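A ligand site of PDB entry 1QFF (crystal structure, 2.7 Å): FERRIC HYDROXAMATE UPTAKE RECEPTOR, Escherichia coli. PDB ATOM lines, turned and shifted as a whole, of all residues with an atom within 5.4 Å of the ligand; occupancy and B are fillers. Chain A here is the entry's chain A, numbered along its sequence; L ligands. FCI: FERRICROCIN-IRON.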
ATOM      1  N   ARG A  81      -3.837 -28.535  12.746  1.00  0.00           N
ATOM      2  CA  ARG A  81      -3.226 -27.214  12.637  1.00  0.00           C
ATOM      3  C   ARG A  81      -3.095 -26.553  14.001  1.00  0.00           C
ATOM      4  O   ARG A  81      -2.738 -25.374  14.110  1.00  0.00           O
ATOM      5  CB  ARG A  81      -4.058 -26.319  11.727  1.00  0.00           C
ATOM      6  CG  ARG A  81      -3.226 -25.298  10.983  1.00  0.00           C
ATOM      7  CD  ARG A  81      -2.331 -25.997   9.995  1.00  0.00           C
ATOM      8  NE  ARG A  81      -1.457 -25.065   9.280  1.00  0.00           N
ATOM      9  CZ  ARG A  81      -0.876 -25.340   8.126  1.00  0.00           C
ATOM     10  NH1 ARG A  81      -1.072 -26.524   7.545  1.00  0.00           N
ATOM     11  NH2 ARG A  81      -0.088 -24.443   7.553  1.00  0.00           N
ATOM     12  N   TYR A  87      -8.866 -22.803   8.685  1.00  0.00           N
ATOM     13  CA  TYR A  87      -9.663 -23.764   7.933  1.00  0.00           C
ATOM     14  C   TYR A  87     -10.176 -24.873   8.823  1.00  0.00           C
ATOM     15  O   TYR A  87      -9.497 -25.283   9.753  1.00  0.00           O
ATOM     16  CB  TYR A  87      -8.836 -24.435   6.840  1.00  0.00           C
ATOM     17  CG  TYR A  87      -8.232 -23.495   5.828  1.00  0.00           C
ATOM     18  CD1 TYR A  87      -9.036 -22.863   4.887  1.00  0.00           C
ATOM     19  CD2 TYR A  87      -6.872 -23.263   5.806  1.00  0.00           C
ATOM     20  CE1 TYR A  87      -8.479 -22.010   3.933  1.00  0.00           C
ATOM     21  CE2 TYR A  87      -6.301 -22.407   4.854  1.00  0.00           C
ATOM     22  CZ  TYR A  87      -7.118 -21.788   3.921  1.00  0.00           C
ATOM     23  OH  TYR A  87      -6.563 -20.937   2.985  1.00  0.00           O
ATOM     24  N   GLU A  98      -7.061 -34.914  -0.565  1.00  0.00           N
ATOM     25  CA  GLU A  98      -5.689 -34.750  -1.049  1.00  0.00           C
ATOM     26  C   GLU A  98      -5.399 -33.259  -1.213  1.00  0.00           C
ATOM     27  O   GLU A  98      -6.292 -32.484  -1.544  1.00  0.00           O
ATOM     28  CB  GLU A  98      -5.511 -35.455  -2.400  1.00  0.00           C
ATOM     29  CG  GLU A  98      -6.091 -36.862  -2.457  1.00  0.00           C
ATOM     30  CD  GLU A  98      -5.114 -37.951  -2.034  1.00  0.00           C
ATOM     31  OE1 GLU A  98      -4.400 -37.747  -1.033  1.00  0.00           O
ATOM     32  OE2 GLU A  98      -5.082 -39.001  -2.702  1.00  0.00           O
ATOM     33  N   GLY A  99      -4.155 -32.877  -0.971  1.00  0.00           N
ATOM     34  CA  GLY A  99      -3.769 -31.482  -1.128  1.00  0.00           C
ATOM     35  C   GLY A  99      -4.219 -30.532  -0.040  1.00  0.00           C
ATOM     36  O   GLY A  99      -4.514 -29.374  -0.332  1.00  0.00           O
ATOM     37  N   GLN A 100      -4.267 -30.998   1.210  1.00  0.00           N
ATOM     38  CA  GLN A 100      -4.687 -30.156   2.329  1.00  0.00           C
ATOM     39  C   GLN A 100      -6.001 -29.442   2.062  1.00  0.00           C
ATOM     40  O   GLN A 100      -6.212 -28.335   2.522  1.00  0.00           O
ATOM     41  CB  GLN A 100      -3.618 -29.118   2.659  1.00  0.00           C
ATOM     42  CG  GLN A 100      -2.675 -29.528   3.776  1.00  0.00           C
ATOM     43  CD  GLN A 100      -3.374 -29.655   5.100  1.00  0.00           C
ATOM     44  OE1 GLN A 100      -4.061 -28.742   5.540  1.00  0.00           O
ATOM     45  NE2 GLN A 100      -3.183 -30.795   5.765  1.00  0.00           N
ATOM     46  N   PHE A 115      -7.008 -25.086  -3.521  1.00  0.00           N
ATOM     47  CA  PHE A 115      -5.798 -24.406  -3.095  1.00  0.00           C
ATOM     48  C   PHE A 115      -6.089 -23.711  -1.764  1.00  0.00           C
ATOM     49  O   PHE A 115      -6.586 -24.349  -0.853  1.00  0.00           O
ATOM     50  CB  PHE A 115      -5.353 -23.418  -4.185  1.00  0.00           C
ATOM     51  CG  PHE A 115      -3.866 -23.317  -4.315  1.00  0.00           C
ATOM     52  CD1 PHE A 115      -3.098 -24.473  -4.474  1.00  0.00           C
ATOM     53  CD2 PHE A 115      -3.214 -22.088  -4.220  1.00  0.00           C
ATOM     54  CE1 PHE A 115      -1.713 -24.404  -4.528  1.00  0.00           C
ATOM     55  CE2 PHE A 115      -1.831 -22.012  -4.266  1.00  0.00           C
ATOM     56  CZ  PHE A 115      -1.077 -23.170  -4.426  1.00  0.00           C
ATOM     57  N   TYR A 116      -5.789 -22.425  -1.634  1.00  0.00           N
ATOM     58  CA  TYR A 116      -6.074 -21.715  -0.389  1.00  0.00           C
ATOM     59  C   TYR A 116      -7.501 -21.218  -0.353  1.00  0.00           C
ATOM     60  O   TYR A 116      -7.898 -20.522   0.572  1.00  0.00           O
ATOM     61  CB  TYR A 116      -5.145 -20.509  -0.209  1.00  0.00           C
ATOM     62  CG  TYR A 116      -3.706 -20.885   0.012  1.00  0.00           C
ATOM     63  CD1 TYR A 116      -3.316 -21.544   1.186  1.00  0.00           C
ATOM     64  CD2 TYR A 116      -2.735 -20.646  -0.960  1.00  0.00           C
ATOM     65  CE1 TYR A 116      -1.994 -21.943   1.384  1.00  0.00           C
ATOM     66  CE2 TYR A 116      -1.411 -21.052  -0.770  1.00  0.00           C
ATOM     67  CZ  TYR A 116      -1.051 -21.700   0.399  1.00  0.00           C
ATOM     68  OH  TYR A 116       0.239 -22.151   0.569  1.00  0.00           O
ATOM     69  N   TYR A 244      -0.853 -19.257  10.274  1.00  0.00           N
ATOM     70  CA  TYR A 244      -0.924 -20.442   9.425  1.00  0.00           C
ATOM     71  C   TYR A 244       0.481 -20.893   9.061  1.00  0.00           C
ATOM     72  O   TYR A 244       0.713 -21.471   7.987  1.00  0.00           O
ATOM     73  CB  TYR A 244      -1.736 -20.118   8.155  1.00  0.00           C
ATOM     74  CG  TYR A 244      -2.336 -21.351   7.499  1.00  0.00           C
ATOM     75  CD1 TYR A 244      -3.183 -22.194   8.219  1.00  0.00           C
ATOM     76  CD2 TYR A 244      -2.031 -21.688   6.188  1.00  0.00           C
ATOM     77  CE1 TYR A 244      -3.702 -23.347   7.634  1.00  0.00           C
ATOM     78  CE2 TYR A 244      -2.551 -22.831   5.593  1.00  0.00           C
ATOM     79  CZ  TYR A 244      -3.388 -23.658   6.328  1.00  0.00           C
ATOM     80  OH  TYR A 244      -3.881 -24.809   5.763  1.00  0.00           O
ATOM     81  N   GLY A 245       1.428 -20.646   9.966  1.00  0.00           N
ATOM     82  CA  GLY A 245       2.802 -21.012   9.698  1.00  0.00           C
ATOM     83  C   GLY A 245       3.211 -22.370  10.222  1.00  0.00           C
ATOM     84  O   GLY A 245       2.435 -23.052  10.885  1.00  0.00           O
ATOM     85  N   TRP A 246       4.447 -22.748   9.913  1.00  0.00           N
ATOM     86  CA  TRP A 246       5.009 -24.031  10.360  1.00  0.00           C
ATOM     87  C   TRP A 246       6.162 -23.762  11.328  1.00  0.00           C
ATOM     88  O   TRP A 246       6.923 -22.803  11.162  1.00  0.00           O
ATOM     89  CB  TRP A 246       5.597 -24.824   9.195  1.00  0.00           C
ATOM     90  CG  TRP A 246       4.689 -25.172   8.071  1.00  0.00           C
ATOM     91  CD1 TRP A 246       3.328 -25.091   8.051  1.00  0.00           C
ATOM     92  CD2 TRP A 246       5.079 -25.685   6.800  1.00  0.00           C
ATOM     93  NE1 TRP A 246       2.849 -25.536   6.838  1.00  0.00           N
ATOM     94  CE2 TRP A 246       3.904 -25.903   6.050  1.00  0.00           C
ATOM     95  CE3 TRP A 246       6.322 -26.007   6.220  1.00  0.00           C
ATOM     96  CZ2 TRP A 246       3.928 -26.420   4.756  1.00  0.00           C
ATOM     97  CZ3 TRP A 246       6.345 -26.516   4.933  1.00  0.00           C
ATOM     98  CH2 TRP A 246       5.156 -26.713   4.215  1.00  0.00           C
ATOM     99  N   TYR A 275      -3.376 -12.263   5.857  1.00  0.00           N
ATOM    100  CA  TYR A 275      -4.165 -13.371   5.298  1.00  0.00           C
ATOM    101  C   TYR A 275      -5.642 -12.979   5.382  1.00  0.00           C
ATOM    102  O   TYR A 275      -6.160 -12.696   6.459  1.00  0.00           O
ATOM    103  CB  TYR A 275      -3.903 -14.628   6.129  1.00  0.00           C
ATOM    104  CG  TYR A 275      -3.945 -15.949   5.381  1.00  0.00           C
ATOM    105  CD1 TYR A 275      -5.085 -16.349   4.679  1.00  0.00           C
ATOM    106  CD2 TYR A 275      -2.857 -16.814   5.421  1.00  0.00           C
ATOM    107  CE1 TYR A 275      -5.136 -17.587   4.033  1.00  0.00           C
ATOM    108  CE2 TYR A 275      -2.901 -18.056   4.781  1.00  0.00           C
ATOM    109  CZ  TYR A 275      -4.032 -18.433   4.101  1.00  0.00           C
ATOM    110  OH  TYR A 275      -4.073 -19.664   3.480  1.00  0.00           O
ATOM    111  N   TYR A 313       6.190 -18.183   5.924  1.00  0.00           N
ATOM    112  CA  TYR A 313       6.005 -19.334   6.785  1.00  0.00           C
ATOM    113  C   TYR A 313       7.375 -19.915   7.049  1.00  0.00           C
ATOM    114  O   TYR A 313       8.332 -19.616   6.345  1.00  0.00           O
ATOM    115  CB  TYR A 313       5.106 -20.383   6.124  1.00  0.00           C
ATOM    116  CG  TYR A 313       5.602 -20.928   4.784  1.00  0.00           C
ATOM    117  CD1 TYR A 313       5.636 -20.121   3.649  1.00  0.00           C
ATOM    118  CD2 TYR A 313       5.995 -22.263   4.660  1.00  0.00           C
ATOM    119  CE1 TYR A 313       6.035 -20.630   2.421  1.00  0.00           C
ATOM    120  CE2 TYR A 313       6.390 -22.785   3.430  1.00  0.00           C
ATOM    121  CZ  TYR A 313       6.411 -21.954   2.310  1.00  0.00           C
ATOM    122  OH  TYR A 313       6.773 -22.447   1.070  1.00  0.00           O
ATOM    123  N   TYR A 315      10.219 -22.958   7.419  1.00  0.00           N
ATOM    124  CA  TYR A 315      10.585 -24.263   6.911  1.00  0.00           C
ATOM    125  C   TYR A 315      11.347 -24.891   8.067  1.00  0.00           C
ATOM    126  O   TYR A 315      11.361 -24.328   9.166  1.00  0.00           O
ATOM    127  CB  TYR A 315      11.448 -24.161   5.657  1.00  0.00           C
ATOM    128  CG  TYR A 315      10.880 -25.016   4.556  1.00  0.00           C
ATOM    129  CD1 TYR A 315       9.603 -24.750   4.057  1.00  0.00           C
ATOM    130  CD2 TYR A 315      11.550 -26.149   4.102  1.00  0.00           C
ATOM    131  CE1 TYR A 315       8.998 -25.621   3.151  1.00  0.00           C
ATOM    132  CE2 TYR A 315      10.945 -27.019   3.195  1.00  0.00           C
ATOM    133  CZ  TYR A 315       9.670 -26.747   2.733  1.00  0.00           C
ATOM    134  OH  TYR A 315       9.034 -27.621   1.865  1.00  0.00           O
ATOM    135  N   VAL A 346       4.892 -16.847   0.412  1.00  0.00           N
ATOM    136  CA  VAL A 346       3.919 -17.035  -0.631  1.00  0.00           C
ATOM    137  C   VAL A 346       2.959 -15.857  -0.634  1.00  0.00           C
ATOM    138  O   VAL A 346       2.452 -15.459   0.417  1.00  0.00           O
ATOM    139  CB  VAL A 346       3.120 -18.359  -0.441  1.00  0.00           C
ATOM    140  CG1 VAL A 346       2.523 -18.405   0.945  1.00  0.00           C
ATOM    141  CG2 VAL A 346       2.054 -18.467  -1.489  1.00  0.00           C
ATOM    142  N   PHE A 391       5.550 -17.936  -5.045  1.00  0.00           N
ATOM    143  CA  PHE A 391       6.195 -18.708  -3.991  1.00  0.00           C
ATOM    144  C   PHE A 391       7.712 -18.497  -3.877  1.00  0.00           C
ATOM    145  O   PHE A 391       8.438 -18.534  -4.870  1.00  0.00           O
ATOM    146  CB  PHE A 391       5.946 -20.207  -4.183  1.00  0.00           C
ATOM    147  CG  PHE A 391       4.549 -20.626  -3.866  1.00  0.00           C
ATOM    148  CD1 PHE A 391       3.520 -20.410  -4.769  1.00  0.00           C
ATOM    149  CD2 PHE A 391       4.258 -21.278  -2.669  1.00  0.00           C
ATOM    150  CE1 PHE A 391       2.214 -20.840  -4.489  1.00  0.00           C
ATOM    151  CE2 PHE A 391       2.972 -21.702  -2.375  1.00  0.00           C
ATOM    152  CZ  PHE A 391       1.943 -21.486  -3.278  1.00  0.00           C
ATOM    153  N   PHE A 704       3.039 -32.446  10.506  1.00  0.00           N
ATOM    154  CA  PHE A 704       2.736 -33.239   9.315  1.00  0.00           C
ATOM    155  C   PHE A 704       4.076 -33.654   8.725  1.00  0.00           C
ATOM    156  O   PHE A 704       4.146 -34.456   7.803  1.00  0.00           O
ATOM    157  CB  PHE A 704       1.903 -32.420   8.322  1.00  0.00           C
ATOM    158  CG  PHE A 704       2.629 -31.257   7.754  1.00  0.00           C
ATOM    159  CD1 PHE A 704       3.405 -31.411   6.603  1.00  0.00           C
ATOM    160  CD2 PHE A 704       2.568 -30.019   8.369  1.00  0.00           C
ATOM    161  CE1 PHE A 704       4.107 -30.340   6.077  1.00  0.00           C
ATOM    162  CE2 PHE A 704       3.273 -28.925   7.836  1.00  0.00           C
ATOM    163  CZ  PHE A 704       4.044 -29.095   6.700  1.00  0.00           C
HETATM  164  C1  FCI L   1       4.813 -26.775   0.024  1.00  0.00           C
HETATM  165  C2  FCI L   1       3.358 -32.967  -0.930  1.00  0.00           C
HETATM  166  C3  FCI L   1       1.712 -23.387   4.395  1.00  0.00           C
HETATM  167  C4  FCI L   1       1.623 -25.556  -1.045  1.00  0.00           C
HETATM  168  C5  FCI L   1       4.650 -30.338  -1.086  1.00  0.00           C
HETATM  169  C6  FCI L   1      -2.741 -25.153   2.620  1.00  0.00           C
HETATM  170  C7  FCI L   1       0.366 -28.419  -0.962  1.00  0.00           C
HETATM  171  C8  FCI L   1       0.263 -32.126  -0.596  1.00  0.00           C
HETATM  172  C9  FCI L   1       0.340 -27.931   4.592  1.00  0.00           C
HETATM  173  C10 FCI L   1       3.778 -25.650   0.084  1.00  0.00           C
HETATM  174  C11 FCI L   1       4.738 -32.734  -1.555  1.00  0.00           C
HETATM  175  C13 FCI L   1       0.164 -25.997  -1.100  1.00  0.00           C
HETATM  176  C14 FCI L   1       5.347 -29.099  -0.569  1.00  0.00           C
HETATM  177  C16 FCI L   1       0.135 -29.737  -0.219  1.00  0.00           C
HETATM  178  C17 FCI L   1       0.940 -33.328  -1.225  1.00  0.00           C
HETATM  179  C18 FCI L   1       4.117 -24.562   1.104  1.00  0.00           C
HETATM  180  C21 FCI L   1      -0.778 -24.873  -0.653  1.00  0.00           C
HETATM  181  C24 FCI L   1       0.416 -29.590   1.284  1.00  0.00           C
HETATM  182  C25 FCI L   1       3.245 -23.332   0.987  1.00  0.00           C
HETATM  183  C27 FCI L   1      -2.268 -25.167  -0.819  1.00  0.00           C
HETATM  184  C29 FCI L   1       1.880 -29.307   1.600  1.00  0.00           C
HETATM  185  C30 FCI L   1       3.037 -22.699   2.330  1.00  0.00           C
HETATM  186  C32 FCI L   1      -2.782 -26.121   0.260  1.00  0.00           C
HETATM  187  C34 FCI L   1       2.082 -29.028   3.080  1.00  0.00           C
HETATM  188  C35 FCI L   1      -4.080 -24.532   2.482  1.00  0.00           C
HETATM  189  C36 FCI L   1       2.612 -22.686   5.321  1.00  0.00           C
HETATM  190  C37 FCI L   1       0.170 -29.123   5.442  1.00  0.00           C
HETATM  191  C38 FCI L   1       4.645 -32.753  -3.078  1.00  0.00           C
HETATM  192 FE   FCI L   1      -0.072 -25.424   3.358  1.00  0.00          FE
HETATM  193  N1  FCI L   1       2.353 -25.944  -0.009  1.00  0.00           N
HETATM  194  N2  FCI L   1       5.323 -31.482  -1.096  1.00  0.00           N
HETATM  195  N3  FCI L   1      -0.081 -27.279  -0.440  1.00  0.00           N
HETATM  196  N4  FCI L   1       0.757 -30.907  -0.793  1.00  0.00           N
HETATM  197  N5  FCI L   1       1.958 -23.353   3.084  1.00  0.00           N
HETATM  198  N6  FCI L   1      -2.227 -25.849   1.597  1.00  0.00           N
HETATM  199  N7  FCI L   1       4.448 -27.958  -0.445  1.00  0.00           N
HETATM  200  N8  FCI L   1       1.211 -27.951   3.564  1.00  0.00           N
HETATM  201  N9  FCI L   1       2.296 -33.073  -1.719  1.00  0.00           N
HETATM  202  O1  FCI L   1       5.986 -26.591   0.404  1.00  0.00           O
HETATM  203  O2  FCI L   1       3.227 -33.043   0.310  1.00  0.00           O
HETATM  204  O3  FCI L   1       0.723 -24.011   4.826  1.00  0.00           O
HETATM  205  O4  FCI L   1       2.123 -24.851  -1.951  1.00  0.00           O
HETATM  206  O5  FCI L   1       3.474 -30.285  -1.503  1.00  0.00           O
HETATM  207  O6  FCI L   1      -2.097 -25.037   3.689  1.00  0.00           O
HETATM  208  O7  FCI L   1       0.965 -28.414  -2.061  1.00  0.00           O
HETATM  209  O8  FCI L   1      -0.315 -26.890   4.826  1.00  0.00           O
HETATM  210  O10 FCI L   1       1.080 -24.030   2.270  1.00  0.00           O
HETATM  211  O11 FCI L   1      -0.986 -26.403   1.798  1.00  0.00           O
HETATM  212  O14 FCI L   1       1.322 -26.813   2.825  1.00  0.00           O
HETATM  213  O17 FCI L   1      -0.787 -32.249   0.080  1.00  0.00           O
HETATM  214  O18 FCI L   1       5.711 -33.501  -3.653  1.00  0.00           O
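OH of Tyr 244 lies close to O6 of the ligand (2.7 Å). The side-chain hydroxyl (OH) of Tyr 116 lies close to an oxygen (O10) of the ligand, 2.7 Å away.
The side-chain hydroxyl (OH) of Tyr 87 is in hydrogen-bond range of the backbone carbonyl oxygen (O) of Tyr 116 (2.8 Å). The backbone carbonyl oxygen of Tyr 244 lies within hydrogen-bond range of the guanidinium group of Arg 81, at 3.1 Å. OH of Tyr 87 sits at hydrogen-bond distance from OH of Tyr 275 (2.8 Å).
The guanidinium group of Arg 81 sits close to an oxygen (O8) of the ligand, 2.8 Å away. NE1 of Trp 246 lies close to O3 of the ligand, at 3.3 Å. Tyr 87 touches the ligand (CE2 to C35, 3.9 Å). CA of Gly 99 touches O17 of the ligand, 3.3 Å away. CG of Gln 100 touches C37 of the ligand, 3.3 Å away. Phe 115 touches the ligand. Tyr 313 touches the ligand. Tyr 315 touches the ligand. Phe 391 touches the ligand (CE2 to O4, 3.3 Å). Phe 704 touches the ligand (CE1 to C34, 3.8 Å). Within 4 Å of the ligand: Arg 81, Tyr 87, Gly 99, Gln 100, Phe 115, Tyr 116, Tyr 244, Trp 246, Tyr 313, Tyr 315, Phe 391 and Phe 704.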
